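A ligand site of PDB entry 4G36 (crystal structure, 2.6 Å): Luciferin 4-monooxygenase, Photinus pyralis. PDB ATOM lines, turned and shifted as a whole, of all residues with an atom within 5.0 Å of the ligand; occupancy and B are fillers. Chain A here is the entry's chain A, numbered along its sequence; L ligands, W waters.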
ATOM      1  N   SER A 203     -10.718   9.517  11.888  1.00  0.00           N
ATOM      2  CA  SER A 203     -10.968   9.295  10.468  1.00  0.00           C
ATOM      3  C   SER A 203     -11.152  10.579   9.667  1.00  0.00           C
ATOM      4  O   SER A 203     -10.931  10.616   8.452  1.00  0.00           O
ATOM      5  CB  SER A 203     -12.184   8.389  10.310  1.00  0.00           C
ATOM      6  OG  SER A 203     -12.075   7.294  11.200  1.00  0.00           O
ATOM      7  N   ARG A 223       4.398  -2.700  10.716  1.00  0.00           N
ATOM      8  CA  ARG A 223       4.866  -1.475  10.074  1.00  0.00           C
ATOM      9  C   ARG A 223       6.374  -1.375  10.176  1.00  0.00           C
ATOM     10  O   ARG A 223       7.046  -1.000   9.211  1.00  0.00           O
ATOM     11  CB  ARG A 223       4.217  -0.266  10.731  1.00  0.00           C
ATOM     12  CG  ARG A 223       4.825   1.071  10.332  1.00  0.00           C
ATOM     13  CD  ARG A 223       4.814   1.260   8.823  1.00  0.00           C
ATOM     14  NE  ARG A 223       5.641   2.400   8.427  1.00  0.00           N
ATOM     15  CZ  ARG A 223       5.954   2.672   7.168  1.00  0.00           C
ATOM     16  NH1 ARG A 223       5.507   1.883   6.188  1.00  0.00           N
ATOM     17  NH2 ARG A 223       6.712   3.725   6.872  1.00  0.00           N
ATOM     18  N   HIS A 250      -1.668  12.337  12.147  1.00  0.00           N
ATOM     19  CA  HIS A 250      -2.299  11.569  11.090  1.00  0.00           C
ATOM     20  C   HIS A 250      -1.465  10.325  10.808  1.00  0.00           C
ATOM     21  O   HIS A 250      -0.247  10.322  11.051  1.00  0.00           O
ATOM     22  CB  HIS A 250      -2.406  12.428   9.832  1.00  0.00           C
ATOM     23  CG  HIS A 250      -3.210  11.790   8.751  1.00  0.00           C
ATOM     24  ND1 HIS A 250      -2.686  10.863   7.872  1.00  0.00           N
ATOM     25  CD2 HIS A 250      -4.514  11.953   8.390  1.00  0.00           C
ATOM     26  CE1 HIS A 250      -3.620  10.488   7.020  1.00  0.00           C
ATOM     27  NE2 HIS A 250      -4.738  11.128   7.313  1.00  0.00           N
ATOM     28  N   GLY A 251      -2.130   9.278  10.336  1.00  0.00           N
ATOM     29  CA  GLY A 251      -1.507   7.970  10.192  1.00  0.00           C
ATOM     30  C   GLY A 251      -0.295   8.022   9.274  1.00  0.00           C
ATOM     31  O   GLY A 251       0.727   7.367   9.530  1.00  0.00           O
ATOM     32  N   PHE A 252      -0.424   8.807   8.204  1.00  0.00           N
ATOM     33  CA  PHE A 252       0.655   9.040   7.258  1.00  0.00           C
ATOM     34  C   PHE A 252       1.933   9.457   7.998  1.00  0.00           C
ATOM     35  O   PHE A 252       2.977   8.825   7.816  1.00  0.00           O
ATOM     36  CB  PHE A 252       0.234  10.096   6.206  1.00  0.00           C
ATOM     37  CG  PHE A 252       1.166  10.219   5.010  1.00  0.00           C
ATOM     38  CD1 PHE A 252       2.354   9.494   4.944  1.00  0.00           C
ATOM     39  CD2 PHE A 252       0.860  11.081   3.970  1.00  0.00           C
ATOM     40  CE1 PHE A 252       3.221   9.633   3.852  1.00  0.00           C
ATOM     41  CE2 PHE A 252       1.716  11.233   2.892  1.00  0.00           C
ATOM     42  CZ  PHE A 252       2.904  10.508   2.826  1.00  0.00           C
ATOM     43  N   THR A 256       4.988   6.594   9.358  1.00  0.00           N
ATOM     44  CA  THR A 256       6.261   6.835   8.696  1.00  0.00           C
ATOM     45  C   THR A 256       7.300   7.274   9.724  1.00  0.00           C
ATOM     46  O   THR A 256       8.404   6.760   9.747  1.00  0.00           O
ATOM     47  CB  THR A 256       6.151   7.937   7.673  1.00  0.00           C
ATOM     48  OG1 THR A 256       5.426   9.016   8.258  1.00  0.00           O
ATOM     49  CG2 THR A 256       5.404   7.436   6.435  1.00  0.00           C
ATOM     50  N   LEU A 291       9.274  13.317   2.151  1.00  0.00           N
ATOM     51  CA  LEU A 291       7.904  12.845   2.326  1.00  0.00           C
ATOM     52  C   LEU A 291       6.880  13.961   2.142  1.00  0.00           C
ATOM     53  O   LEU A 291       6.713  14.795   3.019  1.00  0.00           O
ATOM     54  CB  LEU A 291       7.727  12.249   3.729  1.00  0.00           C
ATOM     55  CG  LEU A 291       6.487  11.405   3.997  1.00  0.00           C
ATOM     56  CD1 LEU A 291       6.479  10.187   3.093  1.00  0.00           C
ATOM     57  CD2 LEU A 291       6.388  10.990   5.473  1.00  0.00           C
ATOM     58  N   ALA A 318       8.553  10.630  -1.826  1.00  0.00           N
ATOM     59  CA  ALA A 318       7.387   9.777  -1.641  1.00  0.00           C
ATOM     60  C   ALA A 318       6.123  10.603  -1.405  1.00  0.00           C
ATOM     61  O   ALA A 318       6.155  11.579  -0.671  1.00  0.00           O
ATOM     62  CB  ALA A 318       7.620   8.839  -0.479  1.00  0.00           C
ATOM     63  N   SER A 319       5.019  10.187  -2.024  1.00  0.00           N
ATOM     64  CA  SER A 319       3.724  10.825  -1.810  1.00  0.00           C
ATOM     65  C   SER A 319       2.695   9.829  -1.298  1.00  0.00           C
ATOM     66  O   SER A 319       2.914   8.614  -1.342  1.00  0.00           O
ATOM     67  CB  SER A 319       3.208  11.471  -3.106  1.00  0.00           C
ATOM     68  OG  SER A 319       1.821  11.765  -3.006  1.00  0.00           O
ATOM     69  N   GLY A 320       1.572  10.335  -0.797  1.00  0.00           N
ATOM     70  CA  GLY A 320       0.541   9.474  -0.252  1.00  0.00           C
ATOM     71  C   GLY A 320      -0.610  10.271   0.299  1.00  0.00           C
ATOM     72  O   GLY A 320      -0.546  11.488   0.369  1.00  0.00           O
ATOM     73  N   GLY A 321      -1.685   9.579   0.677  1.00  0.00           N
ATOM     74  CA  GLY A 321      -2.821  10.242   1.296  1.00  0.00           C
ATOM     75  C   GLY A 321      -3.827  10.830   0.331  1.00  0.00           C
ATOM     76  O   GLY A 321      -4.942  11.191   0.735  1.00  0.00           O
ATOM     77  N   ALA A 322      -3.448  10.935  -0.946  1.00  0.00           N
ATOM     78  CA  ALA A 322      -4.323  11.464  -1.992  1.00  0.00           C
ATOM     79  C   ALA A 322      -3.738  11.182  -3.372  1.00  0.00           C
ATOM     80  O   ALA A 322      -2.556  10.871  -3.502  1.00  0.00           O
ATOM     81  CB  ALA A 322      -4.548  12.948  -1.812  1.00  0.00           C
ATOM     82  N   PRO A 323      -4.557  11.284  -4.429  1.00  0.00           N
ATOM     83  CA  PRO A 323      -3.992  10.995  -5.753  1.00  0.00           C
ATOM     84  C   PRO A 323      -3.002  12.055  -6.237  1.00  0.00           C
ATOM     85  O   PRO A 323      -3.106  13.240  -5.891  1.00  0.00           O
ATOM     86  CB  PRO A 323      -5.227  10.949  -6.656  1.00  0.00           C
ATOM     87  CG  PRO A 323      -6.247  11.771  -5.950  1.00  0.00           C
ATOM     88  CD  PRO A 323      -6.016  11.524  -4.490  1.00  0.00           C
ATOM     89  N   ARG A 342       8.001   7.917  -5.726  1.00  0.00           N
ATOM     90  CA  ARG A 342       7.657   6.770  -4.906  1.00  0.00           C
ATOM     91  C   ARG A 342       6.302   7.074  -4.323  1.00  0.00           C
ATOM     92  O   ARG A 342       5.962   8.233  -4.066  1.00  0.00           O
ATOM     93  CB  ARG A 342       8.662   6.585  -3.780  1.00  0.00           C
ATOM     94  CG  ARG A 342       8.482   5.323  -2.979  1.00  0.00           C
ATOM     95  CD  ARG A 342       9.539   4.319  -3.406  1.00  0.00           C
ATOM     96  NE  ARG A 342       9.499   3.047  -2.677  1.00  0.00           N
ATOM     97  CZ  ARG A 342      10.134   2.823  -1.539  1.00  0.00           C
ATOM     98  NH1 ARG A 342      10.858   3.783  -0.968  1.00  0.00           N
ATOM     99  NH2 ARG A 342      10.052   1.634  -0.965  1.00  0.00           N
ATOM    100  N   GLN A 343       5.513   6.035  -4.107  1.00  0.00           N
ATOM    101  CA  GLN A 343       4.133   6.262  -3.747  1.00  0.00           C
ATOM    102  C   GLN A 343       3.586   5.187  -2.834  1.00  0.00           C
ATOM    103  O   GLN A 343       3.950   4.023  -2.949  1.00  0.00           O
ATOM    104  CB  GLN A 343       3.301   6.346  -5.018  1.00  0.00           C
ATOM    105  CG  GLN A 343       1.838   6.331  -4.747  1.00  0.00           C
ATOM    106  CD  GLN A 343       1.177   7.611  -5.101  1.00  0.00           C
ATOM    107  OE1 GLN A 343       0.035   7.865  -4.709  1.00  0.00           O
ATOM    108  NE2 GLN A 343       1.884   8.438  -5.866  1.00  0.00           N
ATOM    109  N   GLY A 344       2.735   5.586  -1.908  1.00  0.00           N
ATOM    110  CA  GLY A 344       2.129   4.625  -1.016  1.00  0.00           C
ATOM    111  C   GLY A 344       0.672   4.925  -0.770  1.00  0.00           C
ATOM    112  O   GLY A 344       0.270   6.081  -0.707  1.00  0.00           O
ATOM    113  N   TYR A 345      -0.123   3.880  -0.632  1.00  0.00           N
ATOM    114  CA  TYR A 345      -1.539   4.052  -0.424  1.00  0.00           C
ATOM    115  C   TYR A 345      -1.966   3.363   0.867  1.00  0.00           C
ATOM    116  O   TYR A 345      -1.594   2.234   1.101  1.00  0.00           O
ATOM    117  CB  TYR A 345      -2.299   3.469  -1.622  1.00  0.00           C
ATOM    118  CG  TYR A 345      -3.745   3.163  -1.338  1.00  0.00           C
ATOM    119  CD1 TYR A 345      -4.739   4.056  -1.677  1.00  0.00           C
ATOM    120  CD2 TYR A 345      -4.121   1.964  -0.741  1.00  0.00           C
ATOM    121  CE1 TYR A 345      -6.064   3.777  -1.437  1.00  0.00           C
ATOM    122  CE2 TYR A 345      -5.443   1.672  -0.481  1.00  0.00           C
ATOM    123  CZ  TYR A 345      -6.407   2.587  -0.838  1.00  0.00           C
ATOM    124  OH  TYR A 345      -7.726   2.305  -0.577  1.00  0.00           O
ATOM    125  N   GLY A 346      -2.760   4.043   1.685  1.00  0.00           N
ATOM    126  CA  GLY A 346      -3.286   3.452   2.890  1.00  0.00           C
ATOM    127  C   GLY A 346      -4.504   4.199   3.401  1.00  0.00           C
ATOM    128  O   GLY A 346      -4.830   5.282   2.920  1.00  0.00           O
ATOM    129  N   LEU A 347      -5.174   3.601   4.387  1.00  0.00           N
ATOM    130  CA  LEU A 347      -6.283   4.241   5.098  1.00  0.00           C
ATOM    131  C   LEU A 347      -5.926   4.247   6.572  1.00  0.00           C
ATOM    132  O   LEU A 347      -5.137   3.417   7.003  1.00  0.00           O
ATOM    133  CB  LEU A 347      -7.583   3.460   4.862  1.00  0.00           C
ATOM    134  CG  LEU A 347      -8.086   3.373   3.422  1.00  0.00           C
ATOM    135  CD1 LEU A 347      -7.681   2.075   2.745  1.00  0.00           C
ATOM    136  CD2 LEU A 347      -9.591   3.543   3.379  1.00  0.00           C
ATOM    137  N   THR A 348      -6.482   5.179   7.344  1.00  0.00           N
ATOM    138  CA  THR A 348      -6.275   5.224   8.798  1.00  0.00           C
ATOM    139  C   THR A 348      -6.563   3.839   9.393  1.00  0.00           C
ATOM    140  O   THR A 348      -5.861   3.382  10.299  1.00  0.00           O
ATOM    141  CB  THR A 348      -7.179   6.292   9.510  1.00  0.00           C
ATOM    142  OG1 THR A 348      -7.003   7.587   8.929  1.00  0.00           O
ATOM    143  CG2 THR A 348      -6.855   6.382  10.999  1.00  0.00           C
ATOM    144  N   GLU A 349      -7.583   3.182   8.854  1.00  0.00           N
ATOM    145  CA  GLU A 349      -8.008   1.867   9.332  1.00  0.00           C
ATOM    146  C   GLU A 349      -7.068   0.688   8.964  1.00  0.00           C
ATOM    147  O   GLU A 349      -7.224  -0.411   9.482  1.00  0.00           O
ATOM    148  CB  GLU A 349      -9.456   1.574   8.893  1.00  0.00           C
ATOM    149  CG  GLU A 349     -10.523   2.520   9.516  1.00  0.00           C
ATOM    150  CD  GLU A 349     -10.678   3.834   8.767  1.00  0.00           C
ATOM    151  OE1 GLU A 349      -9.652   4.337   8.260  1.00  0.00           O
ATOM    152  OE2 GLU A 349     -11.803   4.368   8.673  1.00  0.00           O
ATOM    153  N   THR A 351      -3.657   1.009   9.451  1.00  0.00           N
ATOM    154  CA  THR A 351      -2.423   1.509  10.078  1.00  0.00           C
ATOM    155  C   THR A 351      -1.566   2.441   9.203  1.00  0.00           C
ATOM    156  O   THR A 351      -1.496   3.648   9.443  1.00  0.00           O
ATOM    157  CB  THR A 351      -1.557   0.375  10.630  1.00  0.00           C
ATOM    158  OG1 THR A 351      -2.298  -0.326  11.631  1.00  0.00           O
ATOM    159  CG2 THR A 351      -0.292   0.927  11.275  1.00  0.00           C
ATOM    160  N   SER A 352      -0.927   1.861   8.198  1.00  0.00           N
ATOM    161  CA  SER A 352      -0.059   2.592   7.274  1.00  0.00           C
ATOM    162  C   SER A 352      -0.322   2.122   5.838  1.00  0.00           C
ATOM    163  O   SER A 352      -1.354   1.500   5.555  1.00  0.00           O
ATOM    164  CB  SER A 352       1.402   2.367   7.668  1.00  0.00           C
ATOM    165  OG  SER A 352       2.255   3.160   6.872  1.00  0.00           O
ATOM    166  N   ALA A 353       0.597   2.416   4.931  1.00  0.00           N
ATOM    167  CA  ALA A 353       0.440   2.025   3.538  1.00  0.00           C
ATOM    168  C   ALA A 353       0.478   0.517   3.377  1.00  0.00           C
ATOM    169  O   ALA A 353       1.361  -0.149   3.916  1.00  0.00           O
ATOM    170  CB  ALA A 353       1.520   2.664   2.683  1.00  0.00           C
ATOM    171  N   ILE A 356       2.490  -0.134  -1.793  1.00  0.00           N
ATOM    172  CA  ILE A 356       3.689   0.694  -1.878  1.00  0.00           C
ATOM    173  C   ILE A 356       4.462   0.430  -3.157  1.00  0.00           C
ATOM    174  O   ILE A 356       4.562  -0.707  -3.580  1.00  0.00           O
ATOM    175  CB  ILE A 356       4.619   0.444  -0.665  1.00  0.00           C
ATOM    176  CG1 ILE A 356       3.971   1.004   0.615  1.00  0.00           C
ATOM    177  CG2 ILE A 356       6.008   1.018  -0.907  1.00  0.00           C
ATOM    178  CD1 ILE A 356       4.717   0.696   1.875  1.00  0.00           C
ATOM    179  N   VAL A 367      -0.183   3.136  -7.577  1.00  0.00           N
ATOM    180  CA  VAL A 367       0.130   3.434  -6.187  1.00  0.00           C
ATOM    181  C   VAL A 367       1.055   2.374  -5.595  1.00  0.00           C
ATOM    182  O   VAL A 367       1.504   2.493  -4.468  1.00  0.00           O
ATOM    183  CB  VAL A 367      -1.136   3.580  -5.308  1.00  0.00           C
ATOM    184  CG1 VAL A 367      -1.831   4.900  -5.606  1.00  0.00           C
ATOM    185  CG2 VAL A 367      -2.079   2.411  -5.534  1.00  0.00           C
ATOM    186  N   SER A 425     -12.532  -0.466   1.369  1.00  0.00           N
ATOM    187  CA  SER A 425     -11.972   0.878   1.372  1.00  0.00           C
ATOM    188  C   SER A 425     -12.839   1.982   0.798  1.00  0.00           C
ATOM    189  O   SER A 425     -12.553   3.164   1.005  1.00  0.00           O
ATOM    190  CB  SER A 425     -10.701   0.865   0.547  1.00  0.00           C
ATOM    191  OG  SER A 425     -11.034   0.422  -0.749  1.00  0.00           O
ATOM    192  N   ASP A 427     -12.813   2.892  -2.018  1.00  0.00           N
ATOM    193  CA  ASP A 427     -12.066   3.418  -3.137  1.00  0.00           C
ATOM    194  C   ASP A 427     -12.276   2.511  -4.351  1.00  0.00           C
ATOM    195  O   ASP A 427     -12.237   1.284  -4.227  1.00  0.00           O
ATOM    196  CB  ASP A 427     -10.579   3.450  -2.791  1.00  0.00           C
ATOM    197  CG  ASP A 427     -10.203   4.569  -1.847  1.00  0.00           C
ATOM    198  OD1 ASP A 427     -10.811   5.650  -1.915  1.00  0.00           O
ATOM    199  OD2 ASP A 427      -9.271   4.379  -1.042  1.00  0.00           O
ATOM    200  N   ILE A 439      -5.563   3.625  -8.502  1.00  0.00           N
ATOM    201  CA  ILE A 439      -6.736   4.116  -7.784  1.00  0.00           C
ATOM    202  C   ILE A 439      -7.445   5.130  -8.638  1.00  0.00           C
ATOM    203  O   ILE A 439      -6.903   6.208  -8.885  1.00  0.00           O
ATOM    204  CB  ILE A 439      -6.340   4.780  -6.457  1.00  0.00           C
ATOM    205  CG1 ILE A 439      -5.290   3.936  -5.740  1.00  0.00           C
ATOM    206  CG2 ILE A 439      -7.580   4.989  -5.554  1.00  0.00           C
ATOM    207  CD1 ILE A 439      -5.818   2.601  -5.260  1.00  0.00           C
ATOM    208  N   ARG A 442     -12.355   7.924  -5.120  1.00  0.00           N
ATOM    209  CA  ARG A 442     -13.218   7.448  -4.060  1.00  0.00           C
ATOM    210  C   ARG A 442     -14.544   7.191  -4.747  1.00  0.00           C
ATOM    211  O   ARG A 442     -14.883   7.890  -5.688  1.00  0.00           O
ATOM    212  CB  ARG A 442     -13.348   8.468  -2.935  1.00  0.00           C
ATOM    213  CG  ARG A 442     -12.086   8.635  -2.126  1.00  0.00           C
ATOM    214  CD  ARG A 442     -12.362   8.707  -0.620  1.00  0.00           C
ATOM    215  NE  ARG A 442     -12.122  10.056  -0.085  1.00  0.00           N
ATOM    216  CZ  ARG A 442     -12.190  10.387   1.212  1.00  0.00           C
ATOM    217  NH1 ARG A 442     -12.488   9.462   2.132  1.00  0.00           N
ATOM    218  NH2 ARG A 442     -11.953  11.639   1.581  1.00  0.00           N
ATOM    219  N   THR A 532      -4.291  16.527   4.065  1.00  0.00           N
ATOM    220  CA  THR A 532      -3.380  15.580   3.428  1.00  0.00           C
ATOM    221  C   THR A 532      -3.457  15.538   1.901  1.00  0.00           C
ATOM    222  O   THR A 532      -2.789  14.712   1.272  1.00  0.00           O
ATOM    223  CB  THR A 532      -3.533  14.122   3.976  1.00  0.00           C
ATOM    224  OG1 THR A 532      -4.848  13.612   3.678  1.00  0.00           O
ATOM    225  CG2 THR A 532      -3.266  14.082   5.488  1.00  0.00           C
ATOM    226  N   LYS A 534      -6.505  15.412  -0.107  1.00  0.00           N
ATOM    227  CA  LYS A 534      -7.791  15.010  -0.670  1.00  0.00           C
ATOM    228  C   LYS A 534      -8.660  16.235  -0.886  1.00  0.00           C
ATOM    229  O   LYS A 534      -8.548  17.228  -0.162  1.00  0.00           O
ATOM    230  CB  LYS A 534      -8.510  14.000   0.252  1.00  0.00           C
ATOM    231  CG  LYS A 534      -7.864  12.623   0.312  1.00  0.00           C
ATOM    232  CD  LYS A 534      -8.708  11.628   1.101  1.00  0.00           C
ATOM    233  CE  LYS A 534      -8.295  11.575   2.561  1.00  0.00           C
ATOM    234  NZ  LYS A 534      -6.825  11.264   2.712  1.00  0.00           N
HETATM  235  O1  LIG L   1      -4.408   8.659   3.826  1.00  0.00           O
HETATM  236  C1  LIG L   1      -4.420   7.883   4.777  1.00  0.00           C
HETATM  237  C2  LIG L   1      -3.171   7.138   5.160  1.00  0.00           C
HETATM  238  N1  LIG L   1      -2.112   7.190   4.392  1.00  0.00           N
HETATM  239  C3  LIG L   1      -3.129   6.440   6.335  1.00  0.00           C
HETATM  240  S1  LIG L   1      -1.502   5.791   6.333  1.00  0.00           S
HETATM  241  C4  LIG L   1      -1.040   6.522   4.804  1.00  0.00           C
HETATM  242  C5  LIG L   1       0.163   6.450   4.130  1.00  0.00           C
HETATM  243  S2  LIG L   1       0.458   7.121   2.564  1.00  0.00           S
HETATM  244  C6  LIG L   1       2.140   6.586   2.454  1.00  0.00           C
HETATM  245  C7  LIG L   1       3.165   6.721   1.496  1.00  0.00           C
HETATM  246  C8  LIG L   1       4.417   6.181   1.751  1.00  0.00           C
HETATM  247  O2  LIG L   1       5.452   6.301   0.807  1.00  0.00           O
HETATM  248  C9  LIG L   1       2.333   5.921   3.673  1.00  0.00           C
HETATM  249  N2  LIG L   1       1.299   5.881   4.464  1.00  0.00           N
HETATM  250  C10 LIG L   1       3.627   5.369   3.886  1.00  0.00           C
HETATM  251  C11 LIG L   1       4.632   5.510   2.934  1.00  0.00           C
HETATM  252  N3  LIG L   1      -5.609   7.618   5.590  1.00  0.00           N
HETATM  253  S3  LIG L   1      -7.040   8.385   5.307  1.00  0.00           S
HETATM  254  O3  LIG L   1      -6.994   9.654   5.973  1.00  0.00           O
HETATM  255  O4  LIG L   1      -8.140   7.740   5.983  1.00  0.00           O
HETATM  256  O5  LIG L   1      -7.274   8.623   3.832  1.00  0.00           O
HETATM  257  C12 LIG L   1      -7.085   7.575   2.907  1.00  0.00           C
HETATM  258  C13 LIG L   1      -7.881   7.867   1.658  1.00  0.00           C
HETATM  259  C14 LIG L   1      -8.034   6.627   0.889  1.00  0.00           C
HETATM  260  O6  LIG L   1      -9.236   6.020   1.215  1.00  0.00           O
HETATM  261  C15 LIG L   1      -7.964   7.099  -0.502  1.00  0.00           C
HETATM  262  O7  LIG L   1      -9.167   7.540  -0.998  1.00  0.00           O
HETATM  263  C16 LIG L   1      -7.059   8.254  -0.398  1.00  0.00           C
HETATM  264  O8  LIG L   1      -7.210   8.833   0.889  1.00  0.00           O
HETATM  265  N4  LIG L   1      -5.660   7.940  -0.612  1.00  0.00           N
HETATM  266  C17 LIG L   1      -5.017   7.926  -1.817  1.00  0.00           C
HETATM  267  N5  LIG L   1      -5.409   8.153  -3.087  1.00  0.00           N
HETATM  268  C18 LIG L   1      -4.549   8.048  -4.088  1.00  0.00           C
HETATM  269  N6  LIG L   1      -3.264   7.742  -3.895  1.00  0.00           N
HETATM  270  C19 LIG L   1      -3.663   7.584  -1.559  1.00  0.00           C
HETATM  271  C20 LIG L   1      -2.770   7.505  -2.664  1.00  0.00           C
HETATM  272  N7  LIG L   1      -1.365   7.173  -2.517  1.00  0.00           N
HETATM  273  N8  LIG L   1      -3.555   7.426  -0.250  1.00  0.00           N
HETATM  274  C21 LIG L   1      -4.730   7.641   0.324  1.00  0.00           C
HETATM  275  O   HOH W   1     -11.218   6.697   2.861  1.00  0.00           O
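Water W1 lies within hydrogen-bond range of O6 of the ligand and NH1 of Arg 442.
OG1 of Thr 348 is in hydrogen-bond range of O4 of the ligand (3.2 Å).
The backbone NH (N) of Thr 348 lies within hydrogen-bond range of a nitrogen (N3) of the ligand.
The side-chain amide oxygen (OE1) of Gln 343 sits at hydrogen-bond distance from a nitrogen (N7) of the ligand (2.7 Å).
A ring nitrogen (NE2) of His 250 sits at hydrogen-bond distance from an oxygen (O3) of the ligand, at 3.0 Å.
The backbone carbonyl oxygen of Gly 344 lies within hydrogen-bond range of a nitrogen (N7) of the ligand.
NZ of Lys 534 is in hydrogen-bond range of O5 of the ligand (2.9 Å).
OD1 of Asp 427 is in hydrogen-bond range of O7 of the ligand, at 2.7 Å.
A nitrogen (N8) of the ligand is in hydrogen-bond range of the backbone NH (N) of Gly 321 (3.0 Å).
A sulfur (S1) of the ligand lies close to the backbone NH of Phe 252 (3.7 Å).
O of Arg 342 lies within hydrogen-bond range of N of Ser 319, 3.0 Å away.
The backbone NH (N) of Phe 252 is in hydrogen-bond range of a ring nitrogen (ND1) of His 250, at 3.1 Å.
The backbone NH (N) of Asp 427 lies close to the side-chain hydroxyl (OG) of Ser 425, at 3.3 Å.
NZ of Lys 534 is in hydrogen-bond range of O of Gly 321 (2.7 Å).
NZ of Lys 534 lies within hydrogen-bond range of OG1 of Thr 532, at 3.2 Å.
The side-chain hydroxyl (OH) of Tyr 345 is in hydrogen-bond range of the side-chain carboxylate (OD2) of Asp 427 (2.6 Å).
The backbone carbonyl oxygen (O) of Phe 252 is in hydrogen-bond range of the side-chain hydroxyl (OG1) of Thr 256 (2.5 Å).
O of Ser 319 lies within hydrogen-bond range of N of Gly 344, 3.1 Å away.
The backbone carbonyl oxygen (O) of Ala 322 sits close to a nitrogen (N6) of the ligand.
A sulfur (S1) of the ligand sits close to the backbone carbonyl oxygen (O) of Thr 351 (3.8 Å).
Residues that only touch the ligand: Gly 251 (3.9 Å), Thr 256 (3.7 Å), Ala 318 (3.6 Å), Ser 319 (3.4 Å), Gly 320 (3.7 Å), Pro 323 (3.3 Å), Tyr 345 (3.7 Å), Gly 346 (3.2 Å), Leu 347 (3.3 Å), Ser 352 (3.6 Å), Ala 353 (3.5 Å), Val 367 (3.6 Å) and Arg 442 (3.3 Å).
23 residues have an atom within 4 Å of the ligand: His 250, Gly 251, Phe 252, Thr 256, Ala 318, Ser 319, Gly 320, Gly 321, Ala 322, Pro 323, Gln 343, Gly 344, Tyr 345, Gly 346, Leu 347, Thr 348, Thr 351, Ser 352, Ala 353, Val 367, Asp 427, Arg 442 and Lys 534.
Along chain A the residues within 4 Å of the ligand span positions 250 to 534.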
